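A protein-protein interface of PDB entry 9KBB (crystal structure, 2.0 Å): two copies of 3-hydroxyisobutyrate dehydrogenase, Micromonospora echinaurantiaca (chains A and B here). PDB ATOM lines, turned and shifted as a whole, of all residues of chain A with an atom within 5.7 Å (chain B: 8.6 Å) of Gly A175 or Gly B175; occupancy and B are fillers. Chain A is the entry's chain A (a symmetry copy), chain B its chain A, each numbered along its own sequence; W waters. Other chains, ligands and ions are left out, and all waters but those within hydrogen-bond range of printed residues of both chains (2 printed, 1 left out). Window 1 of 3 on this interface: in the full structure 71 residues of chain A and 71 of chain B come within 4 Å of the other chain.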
ATOM      1  N   LEU A 170      13.819  11.414 -10.851  1.00  0.00           N
ATOM      2  CA  LEU A 170      13.265  12.434  -9.964  1.00  0.00           C
ATOM      3  C   LEU A 170      12.094  11.880  -9.158  1.00  0.00           C
ATOM      4  O   LEU A 170      11.964  12.153  -7.957  1.00  0.00           O
ATOM      5  CB  LEU A 170      12.826  13.648 -10.785  1.00  0.00           C
ATOM      6  CG  LEU A 170      13.922  14.568 -11.323  1.00  0.00           C
ATOM      7  CD1 LEU A 170      13.296  15.788 -11.975  1.00  0.00           C
ATOM      8  CD2 LEU A 170      14.874  14.987 -10.213  1.00  0.00           C
ATOM      9  N   ALA A 171      11.222  11.107  -9.813  1.00  0.00           N
ATOM     10  CA  ALA A 171      10.117  10.469  -9.103  1.00  0.00           C
ATOM     11  C   ALA A 171      10.628   9.556  -7.994  1.00  0.00           C
ATOM     12  O   ALA A 171      10.080   9.545  -6.885  1.00  0.00           O
ATOM     13  CB  ALA A 171       9.248   9.684 -10.085  1.00  0.00           C
ATOM     14  N   ALA A 172      11.688   8.791  -8.268  1.00  0.00           N
ATOM     15  CA  ALA A 172      12.253   7.935  -7.230  1.00  0.00           C
ATOM     16  C   ALA A 172      12.860   8.768  -6.108  1.00  0.00           C
ATOM     17  O   ALA A 172      12.719   8.428  -4.927  1.00  0.00           O
ATOM     18  CB  ALA A 172      13.296   6.992  -7.831  1.00  0.00           C
ATOM     19  N   MET A 173      13.521   9.874  -6.459  1.00  0.00           N
ATOM     20  CA  MET A 173      14.128  10.739  -5.450  1.00  0.00           C
ATOM     21  C   MET A 173      13.072  11.402  -4.573  1.00  0.00           C
ATOM     22  O   MET A 173      13.227  11.465  -3.349  1.00  0.00           O
ATOM     23  CB  MET A 173      14.989  11.807  -6.122  1.00  0.00           C
ATOM     24  CG  MET A 173      15.602  12.795  -5.145  1.00  0.00           C
ATOM     25  SD  MET A 173      16.177  14.295  -5.963  1.00  0.00           S
ATOM     26  CE  MET A 173      14.628  14.984  -6.544  1.00  0.00           C
ATOM     27  N   TYR A 174      11.999  11.914  -5.178  1.00  0.00           N
ATOM     28  CA  TYR A 174      10.965  12.604  -4.410  1.00  0.00           C
ATOM     29  C   TYR A 174      10.192  11.638  -3.530  1.00  0.00           C
ATOM     30  O   TYR A 174       9.717  12.015  -2.454  1.00  0.00           O
ATOM     31  CB  TYR A 174      10.016  13.337  -5.347  1.00  0.00           C
ATOM     32  CG  TYR A 174      10.579  14.647  -5.781  1.00  0.00           C
ATOM     33  CD1 TYR A 174      11.176  15.496  -4.861  1.00  0.00           C
ATOM     34  CD2 TYR A 174      10.566  15.014  -7.112  1.00  0.00           C
ATOM     35  CE1 TYR A 174      11.709  16.693  -5.252  1.00  0.00           C
ATOM     36  CE2 TYR A 174      11.098  16.204  -7.513  1.00  0.00           C
ATOM     37  CZ  TYR A 174      11.669  17.042  -6.583  1.00  0.00           C
ATOM     38  OH  TYR A 174      12.202  18.230  -7.001  1.00  0.00           O
ATOM     39  N   GLY A 175      10.032  10.401  -3.990  1.00  0.00           N
ATOM     40  CA  GLY A 175       9.451   9.385  -3.128  1.00  0.00           C
ATOM     41  C   GLY A 175      10.295   9.124  -1.908  1.00  0.00           C
ATOM     42  O   GLY A 175       9.800   9.148  -0.771  1.00  0.00           O
ATOM     43  N   MET A 176      11.598   8.861  -2.103  1.00  0.00           N
ATOM     44  CA  MET A 176      12.510   8.625  -0.992  1.00  0.00           C
ATOM     45  C   MET A 176      12.552   9.815  -0.034  1.00  0.00           C
ATOM     46  O   MET A 176      12.495   9.645   1.187  1.00  0.00           O
ATOM     47  CB  MET A 176      13.923   8.319  -1.501  1.00  0.00           C
ATOM     48  CG  MET A 176      14.766   7.541  -0.491  1.00  0.00           C
ATOM     49  SD  MET A 176      16.392   6.993  -1.065  1.00  0.00           S
ATOM     50  CE  MET A 176      17.192   8.557  -1.366  1.00  0.00           C
ATOM     51  N   PHE A 177      12.681  11.027  -0.573  1.00  0.00           N
ATOM     52  CA  PHE A 177      12.772  12.205   0.285  1.00  0.00           C
ATOM     53  C   PHE A 177      11.477  12.421   1.060  1.00  0.00           C
ATOM     54  O   PHE A 177      11.502  12.777   2.239  1.00  0.00           O
ATOM     55  CB  PHE A 177      13.120  13.436  -0.550  1.00  0.00           C
ATOM     56  CG  PHE A 177      14.577  13.538  -0.904  1.00  0.00           C
ATOM     57  CD1 PHE A 177      15.511  12.728  -0.288  1.00  0.00           C
ATOM     58  CD2 PHE A 177      15.007  14.431  -1.866  1.00  0.00           C
ATOM     59  CE1 PHE A 177      16.849  12.812  -0.608  1.00  0.00           C
ATOM     60  CE2 PHE A 177      16.348  14.523  -2.196  1.00  0.00           C
ATOM     61  CZ  PHE A 177      17.270  13.710  -1.567  1.00  0.00           C
ATOM     62  N   GLY A 178      10.339  12.198   0.408  1.00  0.00           N
ATOM     63  CA  GLY A 178       9.069  12.357   1.106  1.00  0.00           C
ATOM     64  C   GLY A 178       8.914  11.380   2.241  1.00  0.00           C
ATOM     65  O   GLY A 178       8.387  11.717   3.314  1.00  0.00           O
ATOM     66  N   GLY A 179       9.361  10.136   2.047  1.00  0.00           N
ATOM     67  CA  GLY A 179       9.323   9.168   3.125  1.00  0.00           C
ATOM     68  C   GLY A 179      10.286   9.512   4.247  1.00  0.00           C
ATOM     69  O   GLY A 179       9.949   9.388   5.430  1.00  0.00           O
ATOM     70  N   TYR A 180      11.497   9.947   3.893  1.00  0.00           N
ATOM     71  CA  TYR A 180      12.458  10.381   4.900  1.00  0.00           C
ATOM     72  C   TYR A 180      11.928  11.578   5.685  1.00  0.00           C
ATOM     73  O   TYR A 180      12.039  11.627   6.914  1.00  0.00           O
ATOM     74  CB  TYR A 180      13.793  10.729   4.238  1.00  0.00           C
ATOM     75  CG  TYR A 180      14.781  11.387   5.174  1.00  0.00           C
ATOM     76  CD1 TYR A 180      15.492  10.639   6.104  1.00  0.00           C
ATOM     77  CD2 TYR A 180      14.978  12.759   5.147  1.00  0.00           C
ATOM     78  CE1 TYR A 180      16.388  11.241   6.969  1.00  0.00           C
ATOM     79  CE2 TYR A 180      15.866  13.368   6.006  1.00  0.00           C
ATOM     80  CZ  TYR A 180      16.568  12.606   6.916  1.00  0.00           C
ATOM     81  OH  TYR A 180      17.452  13.216   7.766  1.00  0.00           O
ATOM     82  N   VAL A 258       0.164   5.690  -0.896  1.00  0.00           N
ATOM     83  CA  VAL A 258       0.681   4.327  -0.827  1.00  0.00           C
ATOM     84  C   VAL A 258      -0.311   3.418  -0.113  1.00  0.00           C
ATOM     85  O   VAL A 258      -0.517   2.270  -0.524  1.00  0.00           O
ATOM     86  CB  VAL A 258       2.069   4.295  -0.160  1.00  0.00           C
ATOM     87  CG1 VAL A 258       2.409   2.883   0.286  1.00  0.00           C
ATOM     88  CG2 VAL A 258       3.116   4.794  -1.132  1.00  0.00           C
ATOM     89  N   ALA B 168       8.862   4.815  11.562  1.00  0.00           N
ATOM     90  CA  ALA B 168       9.538   5.859  10.798  1.00  0.00           C
ATOM     91  C   ALA B 168      10.355   5.258   9.657  1.00  0.00           C
ATOM     92  O   ALA B 168      10.335   5.762   8.528  1.00  0.00           O
ATOM     93  CB  ALA B 168      10.421   6.692  11.726  1.00  0.00           C
ATOM     94  N   LEU B 169      11.083   4.175   9.935  1.00  0.00           N
ATOM     95  CA  LEU B 169      11.815   3.476   8.881  1.00  0.00           C
ATOM     96  C   LEU B 169      10.865   2.960   7.807  1.00  0.00           C
ATOM     97  O   LEU B 169      11.182   3.008   6.611  1.00  0.00           O
ATOM     98  CB  LEU B 169      12.620   2.321   9.482  1.00  0.00           C
ATOM     99  CG  LEU B 169      13.778   2.710  10.400  1.00  0.00           C
ATOM    100  CD1 LEU B 169      14.532   1.465  10.847  1.00  0.00           C
ATOM    101  CD2 LEU B 169      14.710   3.684   9.711  1.00  0.00           C
ATOM    102  N   LEU B 170       9.700   2.456   8.217  1.00  0.00           N
ATOM    103  CA  LEU B 170       8.695   2.001   7.260  1.00  0.00           C
ATOM    104  C   LEU B 170       8.220   3.153   6.379  1.00  0.00           C
ATOM    105  O   LEU B 170       8.042   2.991   5.164  1.00  0.00           O
ATOM    106  CB  LEU B 170       7.516   1.374   8.007  1.00  0.00           C
ATOM    107  CG  LEU B 170       7.722  -0.018   8.604  1.00  0.00           C
ATOM    108  CD1 LEU B 170       6.410  -0.535   9.168  1.00  0.00           C
ATOM    109  CD2 LEU B 170       8.271  -0.981   7.562  1.00  0.00           C
ATOM    110  N   ALA B 171       7.995   4.324   6.983  1.00  0.00           N
ATOM    111  CA  ALA B 171       7.617   5.500   6.206  1.00  0.00           C
ATOM    112  C   ALA B 171       8.680   5.841   5.169  1.00  0.00           C
ATOM    113  O   ALA B 171       8.358   6.168   4.021  1.00  0.00           O
ATOM    114  CB  ALA B 171       7.376   6.687   7.138  1.00  0.00           C
ATOM    115  N   ALA B 172       9.958   5.759   5.550  1.00  0.00           N
ATOM    116  CA  ALA B 172      11.021   6.023   4.585  1.00  0.00           C
ATOM    117  C   ALA B 172      11.042   4.962   3.492  1.00  0.00           C
ATOM    118  O   ALA B 172      11.247   5.279   2.314  1.00  0.00           O
ATOM    119  CB  ALA B 172      12.373   6.097   5.295  1.00  0.00           C
ATOM    120  N   MET B 173      10.811   3.701   3.862  1.00  0.00           N
ATOM    121  CA  MET B 173      10.802   2.619   2.881  1.00  0.00           C
ATOM    122  C   MET B 173       9.641   2.761   1.903  1.00  0.00           C
ATOM    123  O   MET B 173       9.818   2.576   0.694  1.00  0.00           O
ATOM    124  CB  MET B 173      10.722   1.267   3.588  1.00  0.00           C
ATOM    125  CG  MET B 173      10.637   0.088   2.636  1.00  0.00           C
ATOM    126  SD  MET B 173      10.050  -1.408   3.453  1.00  0.00           S
ATOM    127  CE  MET B 173       8.380  -0.929   3.888  1.00  0.00           C
ATOM    128  N   TYR B 174       8.445   3.071   2.405  1.00  0.00           N
ATOM    129  CA  TYR B 174       7.275   3.181   1.536  1.00  0.00           C
ATOM    130  C   TYR B 174       7.373   4.392   0.626  1.00  0.00           C
ATOM    131  O   TYR B 174       6.856   4.375  -0.496  1.00  0.00           O
ATOM    132  CB  TYR B 174       6.006   3.253   2.372  1.00  0.00           C
ATOM    133  CG  TYR B 174       5.562   1.900   2.812  1.00  0.00           C
ATOM    134  CD1 TYR B 174       5.549   0.839   1.918  1.00  0.00           C
ATOM    135  CD2 TYR B 174       5.210   1.665   4.126  1.00  0.00           C
ATOM    136  CE1 TYR B 174       5.159  -0.410   2.315  1.00  0.00           C
ATOM    137  CE2 TYR B 174       4.823   0.422   4.534  1.00  0.00           C
ATOM    138  CZ  TYR B 174       4.798  -0.614   3.628  1.00  0.00           C
ATOM    139  OH  TYR B 174       4.412  -1.855   4.053  1.00  0.00           O
ATOM    140  N   GLY B 175       8.006   5.457   1.107  1.00  0.00           N
ATOM    141  CA  GLY B 175       8.282   6.584   0.231  1.00  0.00           C
ATOM    142  C   GLY B 175       9.192   6.209  -0.909  1.00  0.00           C
ATOM    143  O   GLY B 175       8.889   6.474  -2.082  1.00  0.00           O
ATOM    144  N   MET B 176      10.340   5.583  -0.602  1.00  0.00           N
ATOM    145  CA  MET B 176      11.277   5.147  -1.630  1.00  0.00           C
ATOM    146  C   MET B 176      10.625   4.179  -2.615  1.00  0.00           C
ATOM    147  O   MET B 176      10.789   4.310  -3.831  1.00  0.00           O
ATOM    148  CB  MET B 176      12.511   4.493  -1.000  1.00  0.00           C
ATOM    149  CG  MET B 176      13.736   4.521  -1.916  1.00  0.00           C
ATOM    150  SD  MET B 176      15.283   3.918  -1.197  1.00  0.00           S
ATOM    151  CE  MET B 176      14.868   2.214  -0.878  1.00  0.00           C
ATOM    152  N   PHE B 177       9.904   3.182  -2.102  1.00  0.00           N
ATOM    153  CA  PHE B 177       9.289   2.193  -2.985  1.00  0.00           C
ATOM    154  C   PHE B 177       8.223   2.835  -3.868  1.00  0.00           C
ATOM    155  O   PHE B 177       8.110   2.511  -5.050  1.00  0.00           O
ATOM    156  CB  PHE B 177       8.699   1.051  -2.161  1.00  0.00           C
ATOM    157  CG  PHE B 177       9.719   0.050  -1.693  1.00  0.00           C
ATOM    158  CD1 PHE B 177      11.001   0.056  -2.209  1.00  0.00           C
ATOM    159  CD2 PHE B 177       9.399  -0.882  -0.727  1.00  0.00           C
ATOM    160  CE1 PHE B 177      11.944  -0.856  -1.785  1.00  0.00           C
ATOM    161  CE2 PHE B 177      10.338  -1.802  -0.293  1.00  0.00           C
ATOM    162  CZ  PHE B 177      11.613  -1.786  -0.822  1.00  0.00           C
ATOM    163  N   GLY B 178       7.444   3.753  -3.303  1.00  0.00           N
ATOM    164  CA  GLY B 178       6.428   4.424  -4.105  1.00  0.00           C
ATOM    165  C   GLY B 178       7.026   5.240  -5.220  1.00  0.00           C
ATOM    166  O   GLY B 178       6.494   5.287  -6.341  1.00  0.00           O
ATOM    167  N   GLY B 179       8.148   5.914  -4.954  1.00  0.00           N
ATOM    168  CA  GLY B 179       8.826   6.650  -6.004  1.00  0.00           C
ATOM    169  C   GLY B 179       9.431   5.738  -7.054  1.00  0.00           C
ATOM    170  O   GLY B 179       9.349   6.013  -8.256  1.00  0.00           O
ATOM    171  N   TYR B 180      10.049   4.638  -6.616  1.00  0.00           N
ATOM    172  CA  TYR B 180      10.587   3.661  -7.555  1.00  0.00           C
ATOM    173  C   TYR B 180       9.479   3.058  -8.415  1.00  0.00           C
ATOM    174  O   TYR B 180       9.632   2.914  -9.632  1.00  0.00           O
ATOM    175  CB  TYR B 180      11.332   2.559  -6.798  1.00  0.00           C
ATOM    176  CG  TYR B 180      11.741   1.394  -7.670  1.00  0.00           C
ATOM    177  CD1 TYR B 180      12.837   1.486  -8.518  1.00  0.00           C
ATOM    178  CD2 TYR B 180      11.011   0.215  -7.668  1.00  0.00           C
ATOM    179  CE1 TYR B 180      13.206   0.425  -9.325  1.00  0.00           C
ATOM    180  CE2 TYR B 180      11.368  -0.846  -8.470  1.00  0.00           C
ATOM    181  CZ  TYR B 180      12.466  -0.737  -9.298  1.00  0.00           C
ATOM    182  OH  TYR B 180      12.819  -1.796 -10.092  1.00  0.00           O
ATOM    183  N   LEU B 181       8.362   2.676  -7.785  1.00  0.00           N
ATOM    184  CA  LEU B 181       7.276   2.044  -8.531  1.00  0.00           C
ATOM    185  C   LEU B 181       6.666   3.002  -9.549  1.00  0.00           C
ATOM    186  O   LEU B 181       6.283   2.587 -10.648  1.00  0.00           O
ATOM    187  CB  LEU B 181       6.209   1.525  -7.568  1.00  0.00           C
ATOM    188  CG  LEU B 181       6.622   0.338  -6.696  1.00  0.00           C
ATOM    189  CD1 LEU B 181       5.563   0.072  -5.641  1.00  0.00           C
ATOM    190  CD2 LEU B 181       6.881  -0.903  -7.531  1.00  0.00           C
ATOM    191  N   HIS B 182       6.552   4.284  -9.201  1.00  0.00           N
ATOM    192  CA  HIS B 182       6.099   5.261 -10.186  1.00  0.00           C
ATOM    193  C   HIS B 182       7.098   5.361 -11.334  1.00  0.00           C
ATOM    194  O   HIS B 182       6.712   5.386 -12.510  1.00  0.00           O
ATOM    195  CB  HIS B 182       5.885   6.632  -9.538  1.00  0.00           C
ATOM    196  CG  HIS B 182       5.334   7.650 -10.488  1.00  0.00           C
ATOM    197  ND1 HIS B 182       3.986   7.939 -10.584  1.00  0.00           N
ATOM    198  CD2 HIS B 182       5.946   8.408 -11.426  1.00  0.00           C
ATOM    199  CE1 HIS B 182       3.799   8.849 -11.523  1.00  0.00           C
ATOM    200  NE2 HIS B 182       4.973   9.147 -12.052  1.00  0.00           N
ATOM    201  N   LEU B 205      19.760   6.768  -6.347  1.00  0.00           N
ATOM    202  CA  LEU B 205      19.252   6.821  -4.981  1.00  0.00           C
ATOM    203  C   LEU B 205      20.371   6.677  -3.959  1.00  0.00           C
ATOM    204  O   LEU B 205      20.302   7.278  -2.881  1.00  0.00           O
ATOM    205  CB  LEU B 205      18.186   5.748  -4.774  1.00  0.00           C
ATOM    206  CG  LEU B 205      16.917   5.982  -5.591  1.00  0.00           C
ATOM    207  CD1 LEU B 205      16.030   4.749  -5.554  1.00  0.00           C
ATOM    208  CD2 LEU B 205      16.183   7.205  -5.062  1.00  0.00           C
ATOM    209  N   PHE B 238       8.765  19.988 -10.824  1.00  0.00           N
ATOM    210  CA  PHE B 238       7.835  18.887 -10.598  1.00  0.00           C
ATOM    211  C   PHE B 238       6.774  18.808 -11.685  1.00  0.00           C
ATOM    212  O   PHE B 238       6.263  17.718 -11.974  1.00  0.00           O
ATOM    213  CB  PHE B 238       7.178  19.039  -9.225  1.00  0.00           C
ATOM    214  CG  PHE B 238       6.816  17.737  -8.588  1.00  0.00           C
ATOM    215  CD1 PHE B 238       5.641  17.086  -8.923  1.00  0.00           C
ATOM    216  CD2 PHE B 238       7.664  17.150  -7.670  1.00  0.00           C
ATOM    217  CE1 PHE B 238       5.314  15.879  -8.338  1.00  0.00           C
ATOM    218  CE2 PHE B 238       7.343  15.946  -7.086  1.00  0.00           C
ATOM    219  CZ  PHE B 238       6.169  15.308  -7.420  1.00  0.00           C
ATOM    220  N   LEU B 241       7.432  16.397 -14.455  1.00  0.00           N
ATOM    221  CA  LEU B 241       7.229  15.022 -14.018  1.00  0.00           C
ATOM    222  C   LEU B 241       5.759  14.637 -14.096  1.00  0.00           C
ATOM    223  O   LEU B 241       5.420  13.530 -14.533  1.00  0.00           O
ATOM    224  CB  LEU B 241       7.755  14.855 -12.594  1.00  0.00           C
ATOM    225  CG  LEU B 241       7.549  13.509 -11.890  1.00  0.00           C
ATOM    226  CD1 LEU B 241       7.896  12.315 -12.784  1.00  0.00           C
ATOM    227  CD2 LEU B 241       8.339  13.466 -10.587  1.00  0.00           C
ATOM    228  N   LEU B 254       0.738   8.953  -6.682  1.00  0.00           N
ATOM    229  CA  LEU B 254       1.851   8.826  -5.748  1.00  0.00           C
ATOM    230  C   LEU B 254       2.656  10.116  -5.613  1.00  0.00           C
ATOM    231  O   LEU B 254       3.375  10.281  -4.621  1.00  0.00           O
ATOM    232  CB  LEU B 254       2.771   7.686  -6.189  1.00  0.00           C
ATOM    233  CG  LEU B 254       2.176   6.276  -6.135  1.00  0.00           C
ATOM    234  CD1 LEU B 254       3.246   5.259  -6.456  1.00  0.00           C
ATOM    235  CD2 LEU B 254       1.564   5.993  -4.768  1.00  0.00           C
ATOM    236  N   LEU B 255       2.546  11.034  -6.576  1.00  0.00           N
ATOM    237  CA  LEU B 255       3.384  12.226  -6.608  1.00  0.00           C
ATOM    238  C   LEU B 255       2.698  13.475  -6.084  1.00  0.00           C
ATOM    239  O   LEU B 255       3.383  14.389  -5.615  1.00  0.00           O
ATOM    240  CB  LEU B 255       3.856  12.499  -8.037  1.00  0.00           C
ATOM    241  CG  LEU B 255       4.675  11.420  -8.735  1.00  0.00           C
ATOM    242  CD1 LEU B 255       4.919  11.857 -10.158  1.00  0.00           C
ATOM    243  CD2 LEU B 255       5.979  11.206  -7.994  1.00  0.00           C
ATOM    244  N   VAL B 258       3.730  15.300  -2.632  1.00  0.00           N
ATOM    245  CA  VAL B 258       5.003  16.014  -2.620  1.00  0.00           C
ATOM    246  C   VAL B 258       4.884  17.325  -3.384  1.00  0.00           C
ATOM    247  O   VAL B 258       5.428  18.351  -2.958  1.00  0.00           O
ATOM    248  CB  VAL B 258       6.138  15.131  -3.171  1.00  0.00           C
ATOM    249  CG1 VAL B 258       7.337  15.984  -3.547  1.00  0.00           C
ATOM    250  CG2 VAL B 258       6.540  14.106  -2.133  1.00  0.00           C
HETATM  251  O   HOH W   1      13.042   7.141   2.202  1.00  0.00           O
HETATM  252  O   HOH W   2      12.891   5.853  -4.725  1.00  0.00           O
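Of the printed residues of chain B, Ala A171 touches Gly B179, His B182 and Leu B241. Of the printed residues of chain B, Tyr A174 touches Phe B238 (3.4 Å) and Val B258 (3.8 Å). Of the printed residues of chain B, Gly A175 touches Gly B175 and Met B176. Of the printed residues of chain A, Ala B171 touches Gly A179. Of the printed residues of chain A, Met B176 touches Gly A175 and Met A176. The nearest printed residue of chain A that does not touch Gly B175 is Gly A179 (4.02 Å).
O of Ala A171 touches CA of Gly B179 (3.3 Å). Ala A171 touches Leu B241 (CA to CD2, 3.8 Å). CA of Ala A172 touches C of Gly B179, at 3.6 Å. CD2 of Leu B205 touches O of Ala A172, 3.7 Å away. Tyr A174 touches Phe B238. Tyr A174 touches Val B258. O of Gly A175 touches N of Met B176 (3.6 Å). O of Gly B175 touches N of Met A176, 3.6 Å away. O of Ala B171 touches CA of Gly A179, 3.3 Å away. Gly A179 touches Ala B172 (C to CA, 3.6 Å).
Ala A172 touches Gly B179, and with the chains exchanged Gly A179 touches Ala B172. Tyr A174 touches Val B258, and with the chains exchanged Val A258 touches Tyr B174. Gly B175 touches its own counterpart, Gly A175. Gly A175 touches Met B176, and with the chains exchanged Met A176 touches Gly B175. Of the 15 pairs that touch across the chains among the printed residues, 10 have their exchanged pair printed and touching as well.
The backbone carbonyl oxygen (O) of Gly A175 lies close to the backbone carbonyl oxygen (O) of Gly B175 (3.1 Å). SD of Met A176 sits close to SD of Met B176 (3.3 Å).
Of the 12 printed residues of chain A, 7 touch a printed residue of chain B. Hydrophobic or aromatic side chains of chain A that line the printed part of chain B: Ala A171, Tyr A174, Met A176 and Val A258. Hydrophobic or aromatic side chains of chain B within 4 Å of the printed part of chain A: Met B176, His B182, Leu B205, Phe B238, Leu B241 and Val B258. Among the printed residues, no Asp or Glu carboxylate lies within 4 Å of a Lys or Arg side-chain nitrogen of the other chain.
Water W1 lies within hydrogen-bond range of the backbone carbonyl oxygen of Ala B172 (2.6 Å) and the backbone carbonyl oxygen of Met A176 (2.8 Å). Water W2 lies within hydrogen-bond range of O of Ala A172 (2.6 Å) and O of Met B176 (2.8 Å).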
